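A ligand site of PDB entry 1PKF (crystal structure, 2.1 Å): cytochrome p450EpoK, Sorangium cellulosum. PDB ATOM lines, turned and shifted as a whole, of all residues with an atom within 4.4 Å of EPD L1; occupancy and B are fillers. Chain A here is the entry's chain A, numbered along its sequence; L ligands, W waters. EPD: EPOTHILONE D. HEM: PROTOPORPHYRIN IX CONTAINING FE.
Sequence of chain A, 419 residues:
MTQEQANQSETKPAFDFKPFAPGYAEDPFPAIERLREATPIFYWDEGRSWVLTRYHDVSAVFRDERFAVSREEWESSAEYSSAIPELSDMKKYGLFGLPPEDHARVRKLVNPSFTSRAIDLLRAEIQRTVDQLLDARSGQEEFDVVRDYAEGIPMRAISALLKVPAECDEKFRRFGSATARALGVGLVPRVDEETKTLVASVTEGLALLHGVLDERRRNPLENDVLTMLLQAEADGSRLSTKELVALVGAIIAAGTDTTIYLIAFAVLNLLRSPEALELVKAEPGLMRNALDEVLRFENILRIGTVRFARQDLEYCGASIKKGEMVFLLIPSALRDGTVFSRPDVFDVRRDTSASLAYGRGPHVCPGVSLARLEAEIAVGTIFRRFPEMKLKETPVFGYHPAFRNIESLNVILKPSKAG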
ATOM      1  N   ARG A  71     -19.903  -3.158   9.692  1.00  0.00           N
ATOM      2  CA  ARG A  71     -18.930  -2.286   9.081  1.00  0.00           C
ATOM      3  C   ARG A  71     -18.349  -1.365  10.133  1.00  0.00           C
ATOM      4  O   ARG A  71     -17.336  -0.711   9.901  1.00  0.00           O
ATOM      5  CB  ARG A  71     -19.534  -1.488   7.931  1.00  0.00           C
ATOM      6  CG  ARG A  71     -19.610  -2.273   6.650  1.00  0.00           C
ATOM      7  CD  ARG A  71     -20.737  -3.286   6.634  1.00  0.00           C
ATOM      8  NE  ARG A  71     -20.976  -3.868   5.302  1.00  0.00           N
ATOM      9  CZ  ARG A  71     -20.970  -5.166   5.007  1.00  0.00           C
ATOM     10  NH1 ARG A  71     -20.734  -6.082   5.908  1.00  0.00           N
ATOM     11  NH2 ARG A  71     -21.215  -5.551   3.776  1.00  0.00           N
ATOM     12  N   MET A  90     -29.794   2.766   8.022  1.00  0.00           N
ATOM     13  CA  MET A  90     -29.726   1.447   7.406  1.00  0.00           C
ATOM     14  C   MET A  90     -28.432   0.718   7.730  1.00  0.00           C
ATOM     15  O   MET A  90     -28.447  -0.511   7.860  1.00  0.00           O
ATOM     16  CB  MET A  90     -29.912   1.495   5.910  1.00  0.00           C
ATOM     17  CG  MET A  90     -30.231   0.131   5.353  1.00  0.00           C
ATOM     18  SD  MET A  90     -30.342   0.062   3.575  1.00  0.00           S
ATOM     19  CE  MET A  90     -32.003   0.653   3.291  1.00  0.00           C
ATOM     20  N   LEU A  95     -29.268  -5.356   8.863  1.00  0.00           N
ATOM     21  CA  LEU A  95     -28.804  -6.659   9.262  1.00  0.00           C
ATOM     22  C   LEU A  95     -27.271  -6.761   9.305  1.00  0.00           C
ATOM     23  O   LEU A  95     -26.716  -7.545  10.072  1.00  0.00           O
ATOM     24  CB  LEU A  95     -29.414  -7.746   8.384  1.00  0.00           C
ATOM     25  CG  LEU A  95     -30.913  -7.921   8.700  1.00  0.00           C
ATOM     26  CD1 LEU A  95     -31.644  -8.682   7.628  1.00  0.00           C
ATOM     27  CD2 LEU A  95     -31.134  -8.595  10.035  1.00  0.00           C
ATOM     28  N   PHE A  96     -26.584  -5.931   8.530  1.00  0.00           N
ATOM     29  CA  PHE A  96     -25.115  -5.984   8.559  1.00  0.00           C
ATOM     30  C   PHE A  96     -24.533  -5.241   9.774  1.00  0.00           C
ATOM     31  O   PHE A  96     -23.511  -5.659  10.319  1.00  0.00           O
ATOM     32  CB  PHE A  96     -24.505  -5.501   7.230  1.00  0.00           C
ATOM     33  CG  PHE A  96     -24.668  -6.498   6.089  1.00  0.00           C
ATOM     34  CD1 PHE A  96     -24.489  -6.096   4.775  1.00  0.00           C
ATOM     35  CD2 PHE A  96     -25.028  -7.818   6.339  1.00  0.00           C
ATOM     36  CE1 PHE A  96     -24.625  -6.987   3.717  1.00  0.00           C
ATOM     37  CE2 PHE A  96     -25.161  -8.724   5.287  1.00  0.00           C
ATOM     38  CZ  PHE A  96     -24.961  -8.324   3.979  1.00  0.00           C
ATOM     39  N   ALA A 180     -28.339  -0.605  -3.224  1.00  0.00           N
ATOM     40  CA  ALA A 180     -27.289  -1.620  -3.250  1.00  0.00           C
ATOM     41  C   ALA A 180     -25.971  -0.946  -3.669  1.00  0.00           C
ATOM     42  O   ALA A 180     -24.960  -1.181  -3.056  1.00  0.00           O
ATOM     43  CB  ALA A 180     -27.666  -2.797  -4.161  1.00  0.00           C
ATOM     44  N   LEU A 183     -24.582   1.713  -0.924  1.00  0.00           N
ATOM     45  CA  LEU A 183     -23.939   1.050   0.192  1.00  0.00           C
ATOM     46  C   LEU A 183     -22.488   0.678  -0.125  1.00  0.00           C
ATOM     47  O   LEU A 183     -21.718   0.414   0.757  1.00  0.00           O
ATOM     48  CB  LEU A 183     -24.721  -0.214   0.579  1.00  0.00           C
ATOM     49  CG  LEU A 183     -26.081   0.039   1.208  1.00  0.00           C
ATOM     50  CD1 LEU A 183     -26.823  -1.296   1.344  1.00  0.00           C
ATOM     51  CD2 LEU A 183     -26.004   0.764   2.527  1.00  0.00           C
ATOM     52  N   GLY A 184     -22.145   0.601  -1.389  1.00  0.00           N
ATOM     53  CA  GLY A 184     -20.760   0.400  -1.760  1.00  0.00           C
ATOM     54  C   GLY A 184     -19.842   1.634  -1.611  1.00  0.00           C
ATOM     55  O   GLY A 184     -18.618   1.498  -1.583  1.00  0.00           O
ATOM     56  N   VAL A 188     -16.329  -0.327  -1.172  1.00  0.00           N
ATOM     57  CA  VAL A 188     -15.742  -1.020  -2.286  1.00  0.00           C
ATOM     58  C   VAL A 188     -15.338   0.025  -3.322  1.00  0.00           C
ATOM     59  O   VAL A 188     -15.917   1.103  -3.385  1.00  0.00           O
ATOM     60  CB  VAL A 188     -16.720  -2.091  -2.864  1.00  0.00           C
ATOM     61  CG1 VAL A 188     -17.233  -2.966  -1.744  1.00  0.00           C
ATOM     62  CG2 VAL A 188     -17.860  -1.477  -3.569  1.00  0.00           C
ATOM     63  N   ALA A 250     -33.584  -3.194   3.301  1.00  0.00           N
ATOM     64  CA  ALA A 250     -32.515  -4.122   2.926  1.00  0.00           C
ATOM     65  C   ALA A 250     -33.053  -5.268   2.097  1.00  0.00           C
ATOM     66  O   ALA A 250     -32.406  -5.728   1.154  1.00  0.00           O
ATOM     67  CB  ALA A 250     -31.803  -4.671   4.177  1.00  0.00           C
ATOM     68  N   ALA A 254     -31.454  -5.913  -1.287  1.00  0.00           N
ATOM     69  CA  ALA A 254     -30.814  -7.215  -1.457  1.00  0.00           C
ATOM     70  C   ALA A 254     -31.510  -8.074  -2.519  1.00  0.00           C
ATOM     71  O   ALA A 254     -30.870  -8.866  -3.195  1.00  0.00           O
ATOM     72  CB  ALA A 254     -30.746  -7.963  -0.132  1.00  0.00           C
ATOM     73  N   THR A 258     -29.907  -8.957  -7.471  1.00  0.00           N
ATOM     74  CA  THR A 258     -29.430 -10.344  -7.363  1.00  0.00           C
ATOM     75  C   THR A 258     -30.290 -11.273  -8.188  1.00  0.00           C
ATOM     76  O   THR A 258     -29.793 -12.055  -8.964  1.00  0.00           O
ATOM     77  CB  THR A 258     -29.468 -10.790  -5.878  1.00  0.00           C
ATOM     78  OG1 THR A 258     -30.720 -10.437  -5.268  1.00  0.00           O
ATOM     79  CG2 THR A 258     -28.452 -10.018  -5.057  1.00  0.00           C
ATOM     80  N   LEU A 301     -21.514 -12.865  -8.290  1.00  0.00           N
ATOM     81  CA  LEU A 301     -20.716 -11.891  -7.567  1.00  0.00           C
ATOM     82  C   LEU A 301     -19.389 -11.629  -8.293  1.00  0.00           C
ATOM     83  O   LEU A 301     -18.812 -12.545  -8.884  1.00  0.00           O
ATOM     84  CB  LEU A 301     -20.478 -12.324  -6.154  1.00  0.00           C
ATOM     85  CG  LEU A 301     -21.722 -12.355  -5.286  1.00  0.00           C
ATOM     86  CD1 LEU A 301     -21.450 -13.034  -3.966  1.00  0.00           C
ATOM     87  CD2 LEU A 301     -22.252 -10.920  -5.056  1.00  0.00           C
ATOM     88  N   GLY A 304     -17.133 -10.910  -3.939  1.00  0.00           N
ATOM     89  CA  GLY A 304     -17.746 -11.779  -2.959  1.00  0.00           C
ATOM     90  C   GLY A 304     -18.386 -10.958  -1.885  1.00  0.00           C
ATOM     91  O   GLY A 304     -19.101 -10.023  -2.164  1.00  0.00           O
ATOM     92  N   THR A 305     -18.160 -11.337  -0.630  1.00  0.00           N
ATOM     93  CA  THR A 305     -18.719 -10.595   0.471  1.00  0.00           C
ATOM     94  C   THR A 305     -17.589 -10.301   1.422  1.00  0.00           C
ATOM     95  O   THR A 305     -16.464 -10.750   1.190  1.00  0.00           O
ATOM     96  CB  THR A 305     -19.907 -11.354   1.103  1.00  0.00           C
ATOM     97  OG1 THR A 305     -20.502 -10.546   2.131  1.00  0.00           O
ATOM     98  CG2 THR A 305     -19.412 -12.636   1.791  1.00  0.00           C
ATOM     99  N   VAL A 306     -17.846  -9.517   2.451  1.00  0.00           N
ATOM    100  CA  VAL A 306     -16.801  -9.008   3.312  1.00  0.00           C
ATOM    101  C   VAL A 306     -17.000  -9.381   4.780  1.00  0.00           C
ATOM    102  O   VAL A 306     -18.129  -9.558   5.251  1.00  0.00           O
ATOM    103  CB  VAL A 306     -16.666  -7.459   3.234  1.00  0.00           C
ATOM    104  CG1 VAL A 306     -16.204  -7.092   1.868  1.00  0.00           C
ATOM    105  CG2 VAL A 306     -17.984  -6.746   3.517  1.00  0.00           C
ATOM    106  N   PHE A 327     -12.236 -10.038   2.035  1.00  0.00           N
ATOM    107  CA  PHE A 327     -13.172 -10.444   1.022  1.00  0.00           C
ATOM    108  C   PHE A 327     -13.112 -11.943   0.863  1.00  0.00           C
ATOM    109  O   PHE A 327     -12.029 -12.508   0.762  1.00  0.00           O
ATOM    110  CB  PHE A 327     -12.805  -9.846  -0.332  1.00  0.00           C
ATOM    111  CG  PHE A 327     -13.552  -8.616  -0.681  1.00  0.00           C
ATOM    112  CD1 PHE A 327     -12.964  -7.369  -0.532  1.00  0.00           C
ATOM    113  CD2 PHE A 327     -14.837  -8.686  -1.198  1.00  0.00           C
ATOM    114  CE1 PHE A 327     -13.676  -6.193  -0.883  1.00  0.00           C
ATOM    115  CE2 PHE A 327     -15.541  -7.506  -1.573  1.00  0.00           C
ATOM    116  CZ  PHE A 327     -14.952  -6.274  -1.401  1.00  0.00           C
ATOM    117  N   PRO A 401     -20.223  -2.612  -8.855  1.00  0.00           N
ATOM    118  CA  PRO A 401     -19.139  -2.935  -7.926  1.00  0.00           C
ATOM    119  C   PRO A 401     -19.314  -4.278  -7.233  1.00  0.00           C
ATOM    120  O   PRO A 401     -18.299  -4.809  -6.735  1.00  0.00           O
ATOM    121  CB  PRO A 401     -19.240  -1.825  -6.885  1.00  0.00           C
ATOM    122  CG  PRO A 401     -20.691  -1.480  -6.914  1.00  0.00           C
ATOM    123  CD  PRO A 401     -21.028  -1.484  -8.380  1.00  0.00           C
ATOM    124  N   ALA A 402     -20.540  -4.779  -7.115  1.00  0.00           N
ATOM    125  CA  ALA A 402     -20.754  -6.098  -6.429  1.00  0.00           C
ATOM    126  C   ALA A 402     -20.981  -7.268  -7.357  1.00  0.00           C
ATOM    127  O   ALA A 402     -20.730  -8.422  -6.972  1.00  0.00           O
ATOM    128  CB  ALA A 402     -21.927  -6.026  -5.501  1.00  0.00           C
ATOM    129  N   PHE A 403     -21.564  -6.999  -8.520  1.00  0.00           N
ATOM    130  CA  PHE A 403     -22.068  -8.023  -9.416  1.00  0.00           C
ATOM    131  C   PHE A 403     -21.385  -8.030 -10.787  1.00  0.00           C
ATOM    132  O   PHE A 403     -20.999  -6.991 -11.320  1.00  0.00           O
ATOM    133  CB  PHE A 403     -23.573  -7.854  -9.629  1.00  0.00           C
ATOM    134  CG  PHE A 403     -24.378  -7.892  -8.361  1.00  0.00           C
ATOM    135  CD1 PHE A 403     -25.201  -6.829  -8.011  1.00  0.00           C
ATOM    136  CD2 PHE A 403     -24.310  -8.986  -7.519  1.00  0.00           C
ATOM    137  CE1 PHE A 403     -25.932  -6.879  -6.858  1.00  0.00           C
ATOM    138  CE2 PHE A 403     -25.020  -9.028  -6.372  1.00  0.00           C
ATOM    139  CZ  PHE A 403     -25.848  -7.987  -6.026  1.00  0.00           C
HETATM  140  C51 EPD L   1     -25.904 -11.009  -2.901  1.00  0.00           C
HETATM  141  C5  EPD L   1     -25.778 -10.057  -1.718  1.00  0.00           C
HETATM  142  C4  EPD L   1     -26.815  -9.256  -1.545  1.00  0.00           C
HETATM  143  C3  EPD L   1     -26.975  -8.406  -0.322  1.00  0.00           C
HETATM  144  C2  EPD L   1     -27.145  -6.903  -0.690  1.00  0.00           C
HETATM  145  C20 EPD L   1     -27.354  -5.962   0.587  1.00  0.00           C
HETATM  146  C21 EPD L   1     -27.117  -4.467   0.374  1.00  0.00           C
HETATM  147  C22 EPD L   1     -27.650  -6.588   1.740  1.00  0.00           C
HETATM  148  C23 EPD L   1     -27.843  -5.923   2.982  1.00  0.00           C
HETATM  149  C24 EPD L   1     -28.276  -6.333   4.125  1.00  0.00           C
HETATM  150  S1  EPD L   1     -28.262  -5.081   5.341  1.00  0.00           S
HETATM  151  C25 EPD L   1     -27.612  -4.051   4.124  1.00  0.00           C
HETATM  152  C27 EPD L   1     -27.329  -2.624   4.522  1.00  0.00           C
HETATM  153  N26 EPD L   1     -27.421  -4.551   2.997  1.00  0.00           N
HETATM  154  C6  EPD L   1     -24.838 -10.389  -0.548  1.00  0.00           C
HETATM  155  C7  EPD L   1     -23.390 -10.625  -0.963  1.00  0.00           C
HETATM  156  C8  EPD L   1     -22.757  -9.260  -1.315  1.00  0.00           C
HETATM  157  C9  EPD L   1     -21.847  -8.435  -0.451  1.00  0.00           C
HETATM  158  C91 EPD L   1     -22.325  -7.714   0.756  1.00  0.00           C
HETATM  159  C10 EPD L   1     -21.607  -7.238  -1.495  1.00  0.00           C
HETATM  160  O10 EPD L   1     -20.957  -7.860  -2.669  1.00  0.00           O
HETATM  161  C11 EPD L   1     -20.908  -5.938  -0.925  1.00  0.00           C
HETATM  162  C28 EPD L   1     -19.473  -6.138  -0.440  1.00  0.00           C
HETATM  163  C12 EPD L   1     -20.909  -4.802  -1.947  1.00  0.00           C
HETATM  164  O12 EPD L   1     -20.072  -4.925  -2.849  1.00  0.00           O
HETATM  165  C13 EPD L   1     -21.954  -3.675  -1.741  1.00  0.00           C
HETATM  166  C30 EPD L   1     -21.814  -2.938  -0.428  1.00  0.00           C
HETATM  167  C29 EPD L   1     -22.021  -2.724  -2.936  1.00  0.00           C
HETATM  168  C14 EPD L   1     -23.408  -4.334  -1.596  1.00  0.00           C
HETATM  169  O14 EPD L   1     -24.420  -3.413  -1.179  1.00  0.00           O
HETATM  170  C15 EPD L   1     -24.021  -4.897  -2.853  1.00  0.00           C
HETATM  171  C16 EPD L   1     -25.367  -5.624  -2.525  1.00  0.00           C
HETATM  172  O16 EPD L   1     -26.138  -5.881  -3.439  1.00  0.00           O
HETATM  173  O1  EPD L   1     -25.699  -6.007  -1.163  1.00  0.00           O
HETATM  174  CHA HEM L   2     -27.749 -12.032   2.690  1.00  0.00           C
HETATM  175  CHB HEM L   2     -26.957 -13.995  -1.537  1.00  0.00           C
HETATM  176  CHC HEM L   2     -31.460 -13.033  -3.071  1.00  0.00           C
HETATM  177  CHD HEM L   2     -32.147 -10.782   1.013  1.00  0.00           C
HETATM  178  C1A HEM L   2     -27.181 -12.744   1.692  1.00  0.00           C
HETATM  179  C2A HEM L   2     -25.856 -13.319   1.734  1.00  0.00           C
HETATM  180  C3A HEM L   2     -25.632 -13.850   0.550  1.00  0.00           C
HETATM  181  C4A HEM L   2     -26.796 -13.627  -0.261  1.00  0.00           C
HETATM  182  CMA HEM L   2     -24.339 -14.579   0.176  1.00  0.00           C
HETATM  183  CAA HEM L   2     -24.897 -13.306   2.931  1.00  0.00           C
HETATM  184  CBA HEM L   2     -23.845 -12.201   2.717  1.00  0.00           C
HETATM  185  CGA HEM L   2     -22.859 -12.232   3.859  1.00  0.00           C
HETATM  186  O1A HEM L   2     -22.006 -11.310   3.955  1.00  0.00           O
HETATM  187  O2A HEM L   2     -22.911 -13.176   4.705  1.00  0.00           O
HETATM  188  C1B HEM L   2     -28.100 -13.832  -2.253  1.00  0.00           C
HETATM  189  C2B HEM L   2     -28.221 -14.280  -3.618  1.00  0.00           C
HETATM  190  C3B HEM L   2     -29.469 -14.046  -3.985  1.00  0.00           C
HETATM  191  C4B HEM L   2     -30.137 -13.390  -2.923  1.00  0.00           C
HETATM  192  CMB HEM L   2     -27.148 -14.982  -4.522  1.00  0.00           C
HETATM  193  CAB HEM L   2     -30.105 -14.267  -5.349  1.00  0.00           C
HETATM  194  CBB HEM L   2     -29.984 -15.395  -6.007  1.00  0.00           C
HETATM  195  C1C HEM L   2     -32.118 -12.393  -2.112  1.00  0.00           C
HETATM  196  C2C HEM L   2     -33.518 -12.014  -2.072  1.00  0.00           C
HETATM  197  C3C HEM L   2     -33.698 -11.380  -0.927  1.00  0.00           C
HETATM  198  C4C HEM L   2     -32.428 -11.380  -0.175  1.00  0.00           C
HETATM  199  CMC HEM L   2     -34.576 -12.250  -3.152  1.00  0.00           C
HETATM  200  CAC HEM L   2     -35.029 -10.795  -0.524  1.00  0.00           C
HETATM  201  CBC HEM L   2     -35.219 -10.521   0.728  1.00  0.00           C
HETATM  202  C1D HEM L   2     -30.996 -10.849   1.748  1.00  0.00           C
HETATM  203  C2D HEM L   2     -30.845 -10.141   2.999  1.00  0.00           C
HETATM  204  C3D HEM L   2     -29.491 -10.536   3.525  1.00  0.00           C
HETATM  205  C4D HEM L   2     -28.964 -11.422   2.528  1.00  0.00           C
HETATM  206  CMD HEM L   2     -31.816  -9.226   3.746  1.00  0.00           C
HETATM  207  CAD HEM L   2     -28.861 -10.100   4.834  1.00  0.00           C
HETATM  208  CBD HEM L   2     -29.008 -11.301   5.758  1.00  0.00           C
HETATM  209  CGD HEM L   2     -28.326 -11.040   7.069  1.00  0.00           C
HETATM  210  O1D HEM L   2     -27.328 -10.294   7.117  1.00  0.00           O
HETATM  211  O2D HEM L   2     -28.772 -11.563   8.106  1.00  0.00           O
HETATM  212  NA  HEM L   2     -27.722 -12.938   0.456  1.00  0.00           N
HETATM  213  NB  HEM L   2     -29.303 -13.244  -1.808  1.00  0.00           N
HETATM  214  NC  HEM L   2     -31.522 -12.018  -0.957  1.00  0.00           N
HETATM  215  ND  HEM L   2     -29.862 -11.624   1.466  1.00  0.00           N
HETATM  216 FE   HEM L   2     -29.700 -12.674  -0.206  1.00  0.00          FE
HETATM  217  O   HOH W   1     -22.214  -3.489   2.357  1.00  0.00           O
HETATM  218  O   HOH W   2     -24.456  -4.126   1.692  1.00  0.00           O
HETATM  219  O   HOH W   3     -18.136  -6.236  -4.203  1.00  0.00           O
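The side-chain hydroxyl of Thr 258 sits at hydrogen-bond distance from the backbone carbonyl oxygen of Ala 254 (2.6 Å).
Water W3 bridges O12 of EPD L1 and O of Pro 401.
An oxygen (O10) of EPD L1 sits at hydrogen-bond distance from the backbone carbonyl oxygen (O) of Gly 304, 2.9 Å away.
The backbone carbonyl oxygen (O) of Ala 180 lies within hydrogen-bond range of an oxygen (O14) of EPD L1 (3.0 Å).
S1 of EPD L1 sits close to N of Phe 96 (3.7 Å).
The backbone NH (N) of Leu 95 lies close to a sulfur (S1) of EPD L1.
An oxygen (O1A) of HEM L2 lies within hydrogen-bond range of the side-chain hydroxyl (OG1) of Thr 305 (2.5 Å).
Merely in contact with EPD L1: Leu 183, Phe 403, Ala 402, Thr 258, Gly 184, Thr 305, Val 188, Ala 250, Ala 254 and Arg 71.
Hydrophobic or aromatic side chains within 4 Å of EPD L1: Phe 96, Ala 180, Leu 183, Val 188, Ala 250, Ala 254, Ala 402 and Phe 403.
14 residues have an atom within 4 Å of EPD L1: Arg 71, Leu 95, Phe 96, Ala 180, Leu 183, Gly 184, Val 188, Ala 250, Ala 254, Thr 258, Gly 304, Thr 305, Ala 402 and Phe 403.
The nearest printed residue that does not touch EPD L1 is Met 90 (4.1 Å).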
